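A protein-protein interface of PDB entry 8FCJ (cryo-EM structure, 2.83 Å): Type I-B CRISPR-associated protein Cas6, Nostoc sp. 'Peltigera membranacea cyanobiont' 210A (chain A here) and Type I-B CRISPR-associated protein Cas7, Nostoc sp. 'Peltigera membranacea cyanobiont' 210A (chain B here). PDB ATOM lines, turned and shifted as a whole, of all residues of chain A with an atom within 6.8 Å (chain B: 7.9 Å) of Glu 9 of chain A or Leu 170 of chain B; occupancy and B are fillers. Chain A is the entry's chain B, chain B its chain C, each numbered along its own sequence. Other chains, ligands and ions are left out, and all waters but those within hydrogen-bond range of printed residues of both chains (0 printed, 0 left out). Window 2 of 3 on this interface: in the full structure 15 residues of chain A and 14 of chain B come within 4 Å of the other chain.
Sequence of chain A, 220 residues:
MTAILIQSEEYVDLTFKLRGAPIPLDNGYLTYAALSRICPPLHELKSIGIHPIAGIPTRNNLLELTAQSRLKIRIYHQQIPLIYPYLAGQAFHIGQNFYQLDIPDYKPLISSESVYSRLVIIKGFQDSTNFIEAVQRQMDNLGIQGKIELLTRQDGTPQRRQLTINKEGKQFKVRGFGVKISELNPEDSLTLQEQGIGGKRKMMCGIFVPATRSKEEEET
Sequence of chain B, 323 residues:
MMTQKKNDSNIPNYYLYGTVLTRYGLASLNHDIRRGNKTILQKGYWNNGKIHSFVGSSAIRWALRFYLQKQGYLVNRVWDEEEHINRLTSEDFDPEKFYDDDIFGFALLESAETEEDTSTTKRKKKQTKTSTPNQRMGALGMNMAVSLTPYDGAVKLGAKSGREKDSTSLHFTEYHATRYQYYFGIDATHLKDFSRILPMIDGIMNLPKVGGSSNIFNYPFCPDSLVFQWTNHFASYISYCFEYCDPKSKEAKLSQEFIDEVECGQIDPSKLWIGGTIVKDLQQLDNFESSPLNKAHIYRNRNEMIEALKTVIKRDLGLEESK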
ATOM      1  N   GLN A   7     -13.326  17.194  30.926  1.00  0.00           N
ATOM      2  CA  GLN A   7     -14.181  17.583  29.813  1.00  0.00           C
ATOM      3  C   GLN A   7     -15.171  18.637  30.289  1.00  0.00           C
ATOM      4  O   GLN A   7     -15.954  18.390  31.211  1.00  0.00           O
ATOM      5  CB  GLN A   7     -14.912  16.368  29.247  1.00  0.00           C
ATOM      6  CG  GLN A   7     -13.994  15.235  28.831  1.00  0.00           C
ATOM      7  CD  GLN A   7     -14.703  14.189  27.995  1.00  0.00           C
ATOM      8  OE1 GLN A   7     -15.930  14.175  27.910  1.00  0.00           O
ATOM      9  NE2 GLN A   7     -13.932  13.307  27.372  1.00  0.00           N
ATOM     10  N   SER A   8     -15.133  19.810  29.665  1.00  0.00           N
ATOM     11  CA  SER A   8     -16.003  20.902  30.076  1.00  0.00           C
ATOM     12  C   SER A   8     -17.456  20.586  29.755  1.00  0.00           C
ATOM     13  O   SER A   8     -17.776  20.066  28.682  1.00  0.00           O
ATOM     14  CB  SER A   8     -15.592  22.201  29.388  1.00  0.00           C
ATOM     15  OG  SER A   8     -16.671  23.118  29.353  1.00  0.00           O
ATOM     16  N   GLU A   9     -18.337  20.904  30.695  1.00  0.00           N
ATOM     17  CA  GLU A   9     -19.771  20.809  30.483  1.00  0.00           C
ATOM     18  C   GLU A   9     -20.321  22.163  30.051  1.00  0.00           C
ATOM     19  O   GLU A   9     -19.650  23.195  30.147  1.00  0.00           O
ATOM     20  CB  GLU A   9     -20.474  20.320  31.752  1.00  0.00           C
ATOM     21  CG  GLU A   9     -20.096  21.084  33.007  1.00  0.00           C
ATOM     22  CD  GLU A   9     -20.786  20.546  34.244  1.00  0.00           C
ATOM     23  OE1 GLU A   9     -21.708  19.717  34.096  1.00  0.00           O
ATOM     24  OE2 GLU A   9     -20.406  20.950  35.363  1.00  0.00           O
ATOM     25  N   GLU A  10     -21.550  22.136  29.533  1.00  0.00           N
ATOM     26  CA  GLU A  10     -22.279  23.325  29.102  1.00  0.00           C
ATOM     27  C   GLU A  10     -21.658  23.970  27.867  1.00  0.00           C
ATOM     28  O   GLU A  10     -22.197  24.949  27.342  1.00  0.00           O
ATOM     29  CB  GLU A  10     -22.374  24.348  30.238  1.00  0.00           C
ATOM     30  CG  GLU A  10     -22.989  23.809  31.517  1.00  0.00           C
ATOM     31  CD  GLU A  10     -23.056  24.853  32.612  1.00  0.00           C
ATOM     32  OE1 GLU A  10     -22.754  26.031  32.330  1.00  0.00           O
ATOM     33  OE2 GLU A  10     -23.410  24.497  33.756  1.00  0.00           O
ATOM     34  N   TYR A  11     -20.538  23.436  27.387  1.00  0.00           N
ATOM     35  CA  TYR A  11     -19.894  23.953  26.186  1.00  0.00           C
ATOM     36  C   TYR A  11     -19.445  22.789  25.319  1.00  0.00           C
ATOM     37  O   TYR A  11     -18.775  21.873  25.801  1.00  0.00           O
ATOM     38  CB  TYR A  11     -18.701  24.849  26.531  1.00  0.00           C
ATOM     39  CG  TYR A  11     -19.050  26.317  26.609  1.00  0.00           C
ATOM     40  CD1 TYR A  11     -19.668  26.847  27.733  1.00  0.00           C
ATOM     41  CD2 TYR A  11     -18.767  27.173  25.554  1.00  0.00           C
ATOM     42  CE1 TYR A  11     -19.990  28.187  27.806  1.00  0.00           C
ATOM     43  CE2 TYR A  11     -19.086  28.515  25.617  1.00  0.00           C
ATOM     44  CZ  TYR A  11     -19.697  29.016  26.746  1.00  0.00           C
ATOM     45  OH  TYR A  11     -20.017  30.351  26.815  1.00  0.00           O
ATOM     46  N   VAL A  12     -19.817  22.831  24.040  1.00  0.00           N
ATOM     47  CA  VAL A  12     -19.481  21.792  23.079  1.00  0.00           C
ATOM     48  C   VAL A  12     -18.933  22.457  21.823  1.00  0.00           C
ATOM     49  O   VAL A  12     -18.908  23.680  21.700  1.00  0.00           O
ATOM     50  CB  VAL A  12     -20.688  20.898  22.729  1.00  0.00           C
ATOM     51  CG1 VAL A  12     -21.313  20.321  23.987  1.00  0.00           C
ATOM     52  CG2 VAL A  12     -21.712  21.684  21.934  1.00  0.00           C
ATOM     53  N   TYR A  76     -22.728  27.372  23.675  1.00  0.00           N
ATOM     54  CA  TYR A  76     -23.431  26.825  24.827  1.00  0.00           C
ATOM     55  C   TYR A  76     -24.361  25.709  24.372  1.00  0.00           C
ATOM     56  O   TYR A  76     -25.121  25.873  23.413  1.00  0.00           O
ATOM     57  CB  TYR A  76     -24.223  27.935  25.517  1.00  0.00           C
ATOM     58  CG  TYR A  76     -24.640  27.641  26.938  1.00  0.00           C
ATOM     59  CD1 TYR A  76     -23.696  27.516  27.947  1.00  0.00           C
ATOM     60  CD2 TYR A  76     -25.979  27.501  27.273  1.00  0.00           C
ATOM     61  CE1 TYR A  76     -24.074  27.252  29.248  1.00  0.00           C
ATOM     62  CE2 TYR A  76     -26.366  27.236  28.572  1.00  0.00           C
ATOM     63  CZ  TYR A  76     -25.410  27.112  29.555  1.00  0.00           C
ATOM     64  OH  TYR A  76     -25.793  26.849  30.850  1.00  0.00           O
ATOM     65  N   HIS A  77     -24.303  24.566  25.061  1.00  0.00           N
ATOM     66  CA  HIS A  77     -25.029  23.389  24.595  1.00  0.00           C
ATOM     67  C   HIS A  77     -26.541  23.569  24.647  1.00  0.00           C
ATOM     68  O   HIS A  77     -27.257  22.859  23.936  1.00  0.00           O
ATOM     69  CB  HIS A  77     -24.618  22.157  25.403  1.00  0.00           C
ATOM     70  CG  HIS A  77     -25.285  22.054  26.738  1.00  0.00           C
ATOM     71  ND1 HIS A  77     -25.843  20.882  27.201  1.00  0.00           N
ATOM     72  CD2 HIS A  77     -25.480  22.973  27.712  1.00  0.00           C
ATOM     73  CE1 HIS A  77     -26.356  21.085  28.402  1.00  0.00           C
ATOM     74  NE2 HIS A  77     -26.149  22.346  28.734  1.00  0.00           N
ATOM     75  N   PRO A 108     -16.563  17.271  22.779  1.00  0.00           N
ATOM     76  CA  PRO A 108     -16.455  17.885  24.104  1.00  0.00           C
ATOM     77  C   PRO A 108     -15.242  18.796  24.197  1.00  0.00           C
ATOM     78  O   PRO A 108     -14.263  18.661  23.460  1.00  0.00           O
ATOM     79  CB  PRO A 108     -16.321  16.683  25.044  1.00  0.00           C
ATOM     80  CG  PRO A 108     -15.724  15.615  24.198  1.00  0.00           C
ATOM     81  CD  PRO A 108     -16.215  15.841  22.795  1.00  0.00           C
ATOM     82  N   LEU A 109     -15.323  19.744  25.127  1.00  0.00           N
ATOM     83  CA  LEU A 109     -14.248  20.702  25.356  1.00  0.00           C
ATOM     84  C   LEU A 109     -13.275  20.104  26.367  1.00  0.00           C
ATOM     85  O   LEU A 109     -13.569  20.044  27.564  1.00  0.00           O
ATOM     86  CB  LEU A 109     -14.814  22.032  25.844  1.00  0.00           C
ATOM     87  CG  LEU A 109     -14.216  23.283  25.202  1.00  0.00           C
ATOM     88  CD1 LEU A 109     -14.089  23.093  23.703  1.00  0.00           C
ATOM     89  CD2 LEU A 109     -15.072  24.495  25.512  1.00  0.00           C
ATOM     90  N   LEU A 190     -10.141  25.230  30.961  1.00  0.00           N
ATOM     91  CA  LEU A 190     -11.482  25.117  30.400  1.00  0.00           C
ATOM     92  C   LEU A 190     -12.208  26.454  30.438  1.00  0.00           C
ATOM     93  O   LEU A 190     -12.928  26.803  29.496  1.00  0.00           O
ATOM     94  CB  LEU A 190     -12.282  24.052  31.148  1.00  0.00           C
ATOM     95  CG  LEU A 190     -11.856  22.608  30.896  1.00  0.00           C
ATOM     96  CD1 LEU A 190     -12.683  21.652  31.739  1.00  0.00           C
ATOM     97  CD2 LEU A 190     -11.976  22.273  29.420  1.00  0.00           C
ATOM     98  N   GLU A 194     -13.636  28.168  27.020  1.00  0.00           N
ATOM     99  CA  GLU A 194     -15.031  28.552  26.821  1.00  0.00           C
ATOM    100  C   GLU A 194     -15.166  30.056  26.622  1.00  0.00           C
ATOM    101  O   GLU A 194     -15.826  30.510  25.680  1.00  0.00           O
ATOM    102  CB  GLU A 194     -15.886  28.095  28.005  1.00  0.00           C
ATOM    103  CG  GLU A 194     -15.768  26.624  28.348  1.00  0.00           C
ATOM    104  CD  GLU A 194     -16.246  26.318  29.753  1.00  0.00           C
ATOM    105  OE1 GLU A 194     -15.705  26.913  30.708  1.00  0.00           O
ATOM    106  OE2 GLU A 194     -17.162  25.482  29.904  1.00  0.00           O
ATOM    107  N   ASN B  37     -18.366   8.520  22.844  1.00  0.00           N
ATOM    108  CA  ASN B  37     -19.178   8.590  24.050  1.00  0.00           C
ATOM    109  C   ASN B  37     -20.623   8.975  23.773  1.00  0.00           C
ATOM    110  O   ASN B  37     -21.480   8.768  24.638  1.00  0.00           O
ATOM    111  CB  ASN B  37     -18.577   9.593  25.040  1.00  0.00           C
ATOM    112  CG  ASN B  37     -17.160   9.242  25.435  1.00  0.00           C
ATOM    113  OD1 ASN B  37     -16.654   8.174  25.091  1.00  0.00           O
ATOM    114  ND2 ASN B  37     -16.507  10.141  26.162  1.00  0.00           N
ATOM    115  N   LYS B  38     -20.909   9.512  22.593  1.00  0.00           N
ATOM    116  CA  LYS B  38     -22.235  10.019  22.293  1.00  0.00           C
ATOM    117  C   LYS B  38     -23.165   8.900  21.844  1.00  0.00           C
ATOM    118  O   LYS B  38     -22.754   7.947  21.179  1.00  0.00           O
ATOM    119  CB  LYS B  38     -22.160  11.091  21.207  1.00  0.00           C
ATOM    120  CG  LYS B  38     -20.877  11.051  20.403  1.00  0.00           C
ATOM    121  CD  LYS B  38     -20.755  12.255  19.489  1.00  0.00           C
ATOM    122  CE  LYS B  38     -19.363  12.335  18.891  1.00  0.00           C
ATOM    123  NZ  LYS B  38     -18.367  12.861  19.864  1.00  0.00           N
ATOM    124  N   LYS B 156     -28.291  16.333  25.544  1.00  0.00           N
ATOM    125  CA  LYS B 156     -28.389  16.243  26.993  1.00  0.00           C
ATOM    126  C   LYS B 156     -27.092  15.689  27.563  1.00  0.00           C
ATOM    127  O   LYS B 156     -26.495  14.771  26.992  1.00  0.00           O
ATOM    128  CB  LYS B 156     -29.569  15.359  27.407  1.00  0.00           C
ATOM    129  CG  LYS B 156     -29.767  15.234  28.906  1.00  0.00           C
ATOM    130  CD  LYS B 156     -31.232  15.026  29.250  1.00  0.00           C
ATOM    131  CE  LYS B 156     -32.046  16.282  28.982  1.00  0.00           C
ATOM    132  NZ  LYS B 156     -33.479  16.103  29.344  1.00  0.00           N
ATOM    133  N   LEU B 157     -26.657  16.255  28.685  1.00  0.00           N
ATOM    134  CA  LEU B 157     -25.437  15.821  29.351  1.00  0.00           C
ATOM    135  C   LEU B 157     -25.768  14.849  30.476  1.00  0.00           C
ATOM    136  O   LEU B 157     -26.638  15.123  31.308  1.00  0.00           O
ATOM    137  CB  LEU B 157     -24.670  17.022  29.903  1.00  0.00           C
ATOM    138  CG  LEU B 157     -23.415  17.406  29.121  1.00  0.00           C
ATOM    139  CD1 LEU B 157     -22.415  16.264  29.147  1.00  0.00           C
ATOM    140  CD2 LEU B 157     -23.770  17.781  27.692  1.00  0.00           C
ATOM    141  N   GLY B 158     -25.072  13.721  30.497  1.00  0.00           N
ATOM    142  CA  GLY B 158     -25.253  12.738  31.549  1.00  0.00           C
ATOM    143  C   GLY B 158     -23.930  12.110  31.923  1.00  0.00           C
ATOM    144  O   GLY B 158     -23.019  11.991  31.101  1.00  0.00           O
ATOM    145  N   ALA B 159     -23.834  11.698  33.184  1.00  0.00           N
ATOM    146  CA  ALA B 159     -22.626  11.092  33.730  1.00  0.00           C
ATOM    147  C   ALA B 159     -22.870   9.599  33.903  1.00  0.00           C
ATOM    148  O   ALA B 159     -23.711   9.192  34.712  1.00  0.00           O
ATOM    149  CB  ALA B 159     -22.238  11.744  35.055  1.00  0.00           C
ATOM    150  N   LYS B 160     -22.134   8.788  33.149  1.00  0.00           N
ATOM    151  CA  LYS B 160     -22.247   7.341  33.239  1.00  0.00           C
ATOM    152  C   LYS B 160     -21.277   6.798  34.280  1.00  0.00           C
ATOM    153  O   LYS B 160     -20.240   7.401  34.570  1.00  0.00           O
ATOM    154  CB  LYS B 160     -21.988   6.692  31.878  1.00  0.00           C
ATOM    155  CG  LYS B 160     -20.550   6.782  31.394  1.00  0.00           C
ATOM    156  CD  LYS B 160     -20.356   5.982  30.115  1.00  0.00           C
ATOM    157  CE  LYS B 160     -18.908   6.013  29.656  1.00  0.00           C
ATOM    158  NZ  LYS B 160     -18.694   5.205  28.423  1.00  0.00           N
ATOM    159  N   SER B 167     -15.043   7.085  38.881  1.00  0.00           N
ATOM    160  CA  SER B 167     -14.970   8.179  37.926  1.00  0.00           C
ATOM    161  C   SER B 167     -16.267   8.289  37.133  1.00  0.00           C
ATOM    162  O   SER B 167     -16.894   7.287  36.777  1.00  0.00           O
ATOM    163  CB  SER B 167     -13.797   7.982  36.966  1.00  0.00           C
ATOM    164  OG  SER B 167     -13.910   6.754  36.268  1.00  0.00           O
ATOM    165  N   THR B 168     -16.666   9.528  36.858  1.00  0.00           N
ATOM    166  CA  THR B 168     -17.846   9.820  36.053  1.00  0.00           C
ATOM    167  C   THR B 168     -17.403  10.565  34.803  1.00  0.00           C
ATOM    168  O   THR B 168     -16.809  11.644  34.897  1.00  0.00           O
ATOM    169  CB  THR B 168     -18.864  10.649  36.838  1.00  0.00           C
ATOM    170  OG1 THR B 168     -18.242  11.849  37.315  1.00  0.00           O
ATOM    171  CG2 THR B 168     -19.397   9.854  38.022  1.00  0.00           C
ATOM    172  N   SER B 169     -17.692   9.991  33.640  1.00  0.00           N
ATOM    173  CA  SER B 169     -17.328  10.583  32.361  1.00  0.00           C
ATOM    174  C   SER B 169     -18.565  11.181  31.710  1.00  0.00           C
ATOM    175  O   SER B 169     -19.615  10.532  31.643  1.00  0.00           O
ATOM    176  CB  SER B 169     -16.692   9.542  31.438  1.00  0.00           C
ATOM    177  OG  SER B 169     -17.573   8.458  31.212  1.00  0.00           O
ATOM    178  N   LEU B 170     -18.440  12.417  31.235  1.00  0.00           N
ATOM    179  CA  LEU B 170     -19.561  13.122  30.629  1.00  0.00           C
ATOM    180  C   LEU B 170     -19.736  12.657  29.190  1.00  0.00           C
ATOM    181  O   LEU B 170     -18.817  12.786  28.374  1.00  0.00           O
ATOM    182  CB  LEU B 170     -19.329  14.629  30.688  1.00  0.00           C
ATOM    183  CG  LEU B 170     -19.693  15.303  32.013  1.00  0.00           C
ATOM    184  CD1 LEU B 170     -19.501  16.805  31.920  1.00  0.00           C
ATOM    185  CD2 LEU B 170     -21.119  14.965  32.414  1.00  0.00           C
ATOM    186  N   HIS B 171     -20.912  12.119  28.878  1.00  0.00           N
ATOM    187  CA  HIS B 171     -21.212  11.636  27.542  1.00  0.00           C
ATOM    188  C   HIS B 171     -22.513  12.262  27.060  1.00  0.00           C
ATOM    189  O   HIS B 171     -23.370  12.661  27.853  1.00  0.00           O
ATOM    190  CB  HIS B 171     -21.305  10.105  27.498  1.00  0.00           C
ATOM    191  CG  HIS B 171     -22.671   9.569  27.788  1.00  0.00           C
ATOM    192  ND1 HIS B 171     -23.353   8.760  26.904  1.00  0.00           N
ATOM    193  CD2 HIS B 171     -23.480   9.718  28.864  1.00  0.00           C
ATOM    194  CE1 HIS B 171     -24.526   8.438  27.421  1.00  0.00           C
ATOM    195  NE2 HIS B 171     -24.627   9.006  28.609  1.00  0.00           N
ATOM    196  N   PHE B 172     -22.648  12.343  25.742  1.00  0.00           N
ATOM    197  CA  PHE B 172     -23.726  13.082  25.101  1.00  0.00           C
ATOM    198  C   PHE B 172     -24.838  12.130  24.689  1.00  0.00           C
ATOM    199  O   PHE B 172     -24.577  11.092  24.074  1.00  0.00           O
ATOM    200  CB  PHE B 172     -23.205  13.839  23.879  1.00  0.00           C
ATOM    201  CG  PHE B 172     -22.256  14.958  24.209  1.00  0.00           C
ATOM    202  CD1 PHE B 172     -21.946  15.268  25.523  1.00  0.00           C
ATOM    203  CD2 PHE B 172     -21.657  15.686  23.200  1.00  0.00           C
ATOM    204  CE1 PHE B 172     -21.070  16.292  25.820  1.00  0.00           C
ATOM    205  CE2 PHE B 172     -20.779  16.709  23.492  1.00  0.00           C
ATOM    206  CZ  PHE B 172     -20.485  17.012  24.803  1.00  0.00           C
ATOM    207  N   THR B 173     -26.074  12.482  25.030  1.00  0.00           N
ATOM    208  CA  THR B 173     -27.248  11.756  24.571  1.00  0.00           C
ATOM    209  C   THR B 173     -28.176  12.734  23.866  1.00  0.00           C
ATOM    210  O   THR B 173     -28.295  13.894  24.276  1.00  0.00           O
ATOM    211  CB  THR B 173     -27.955  11.037  25.733  1.00  0.00           C
ATOM    212  OG1 THR B 173     -28.679   9.907  25.228  1.00  0.00           O
ATOM    213  CG2 THR B 173     -28.912  11.954  26.473  1.00  0.00           C
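The side-chain amide oxygen (OE1) of Gln 7 of chain A lies close to the backbone carbonyl oxygen (O) of Leu 170 of chain B (3.2 Å).
The backbone carbonyl oxygen (O) of Glu 10 of chain A lies within hydrogen-bond range of the backbone NH (N) of His 77 of chain A, at 3.1 Å.
Glu 9 of chain A touches Leu 170 of chain B. Val 12 of chain A touches Phe 172 of chain B (CG1 to CZ, 3.5 Å). ND1 of His 77 of chain A touches CD2 of Leu 157 of chain B (3.8 Å).
Of the printed residues of chain B, Gln 7 of chain A touches Leu 170 (3.2 Å). No residue of chain B comes within 4 Å of Ser 8 of chain A. Glu 9 of chain A touches one residue of chain B. Of the printed residues of chain B, His 77 of chain A touches Leu 157. Printed residues of chain A within 4 Å of Leu 157 of chain B: His 77. Thr 168 of chain B touches none of the printed residues of chain A. Of the printed residues of chain A, Phe 172 of chain B touches Val 12. The nearest residue of chain B that does not touch Glu 9 of chain A is Leu 157 of chain B (4.9 Å). The nearest printed residue of chain A that does not touch Leu 157 of chain B is Glu 9 of chain A (4.9 Å).
Of the 12 printed residues of chain A, 4 touch a printed residue of chain B. Along chain A the printed residues that touch a printed residue of chain B span positions 7 to 77. Of the 14 printed residues of chain B, 3 touch a printed residue of chain A. Among the printed residues, 4 pairs touch across the chains.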
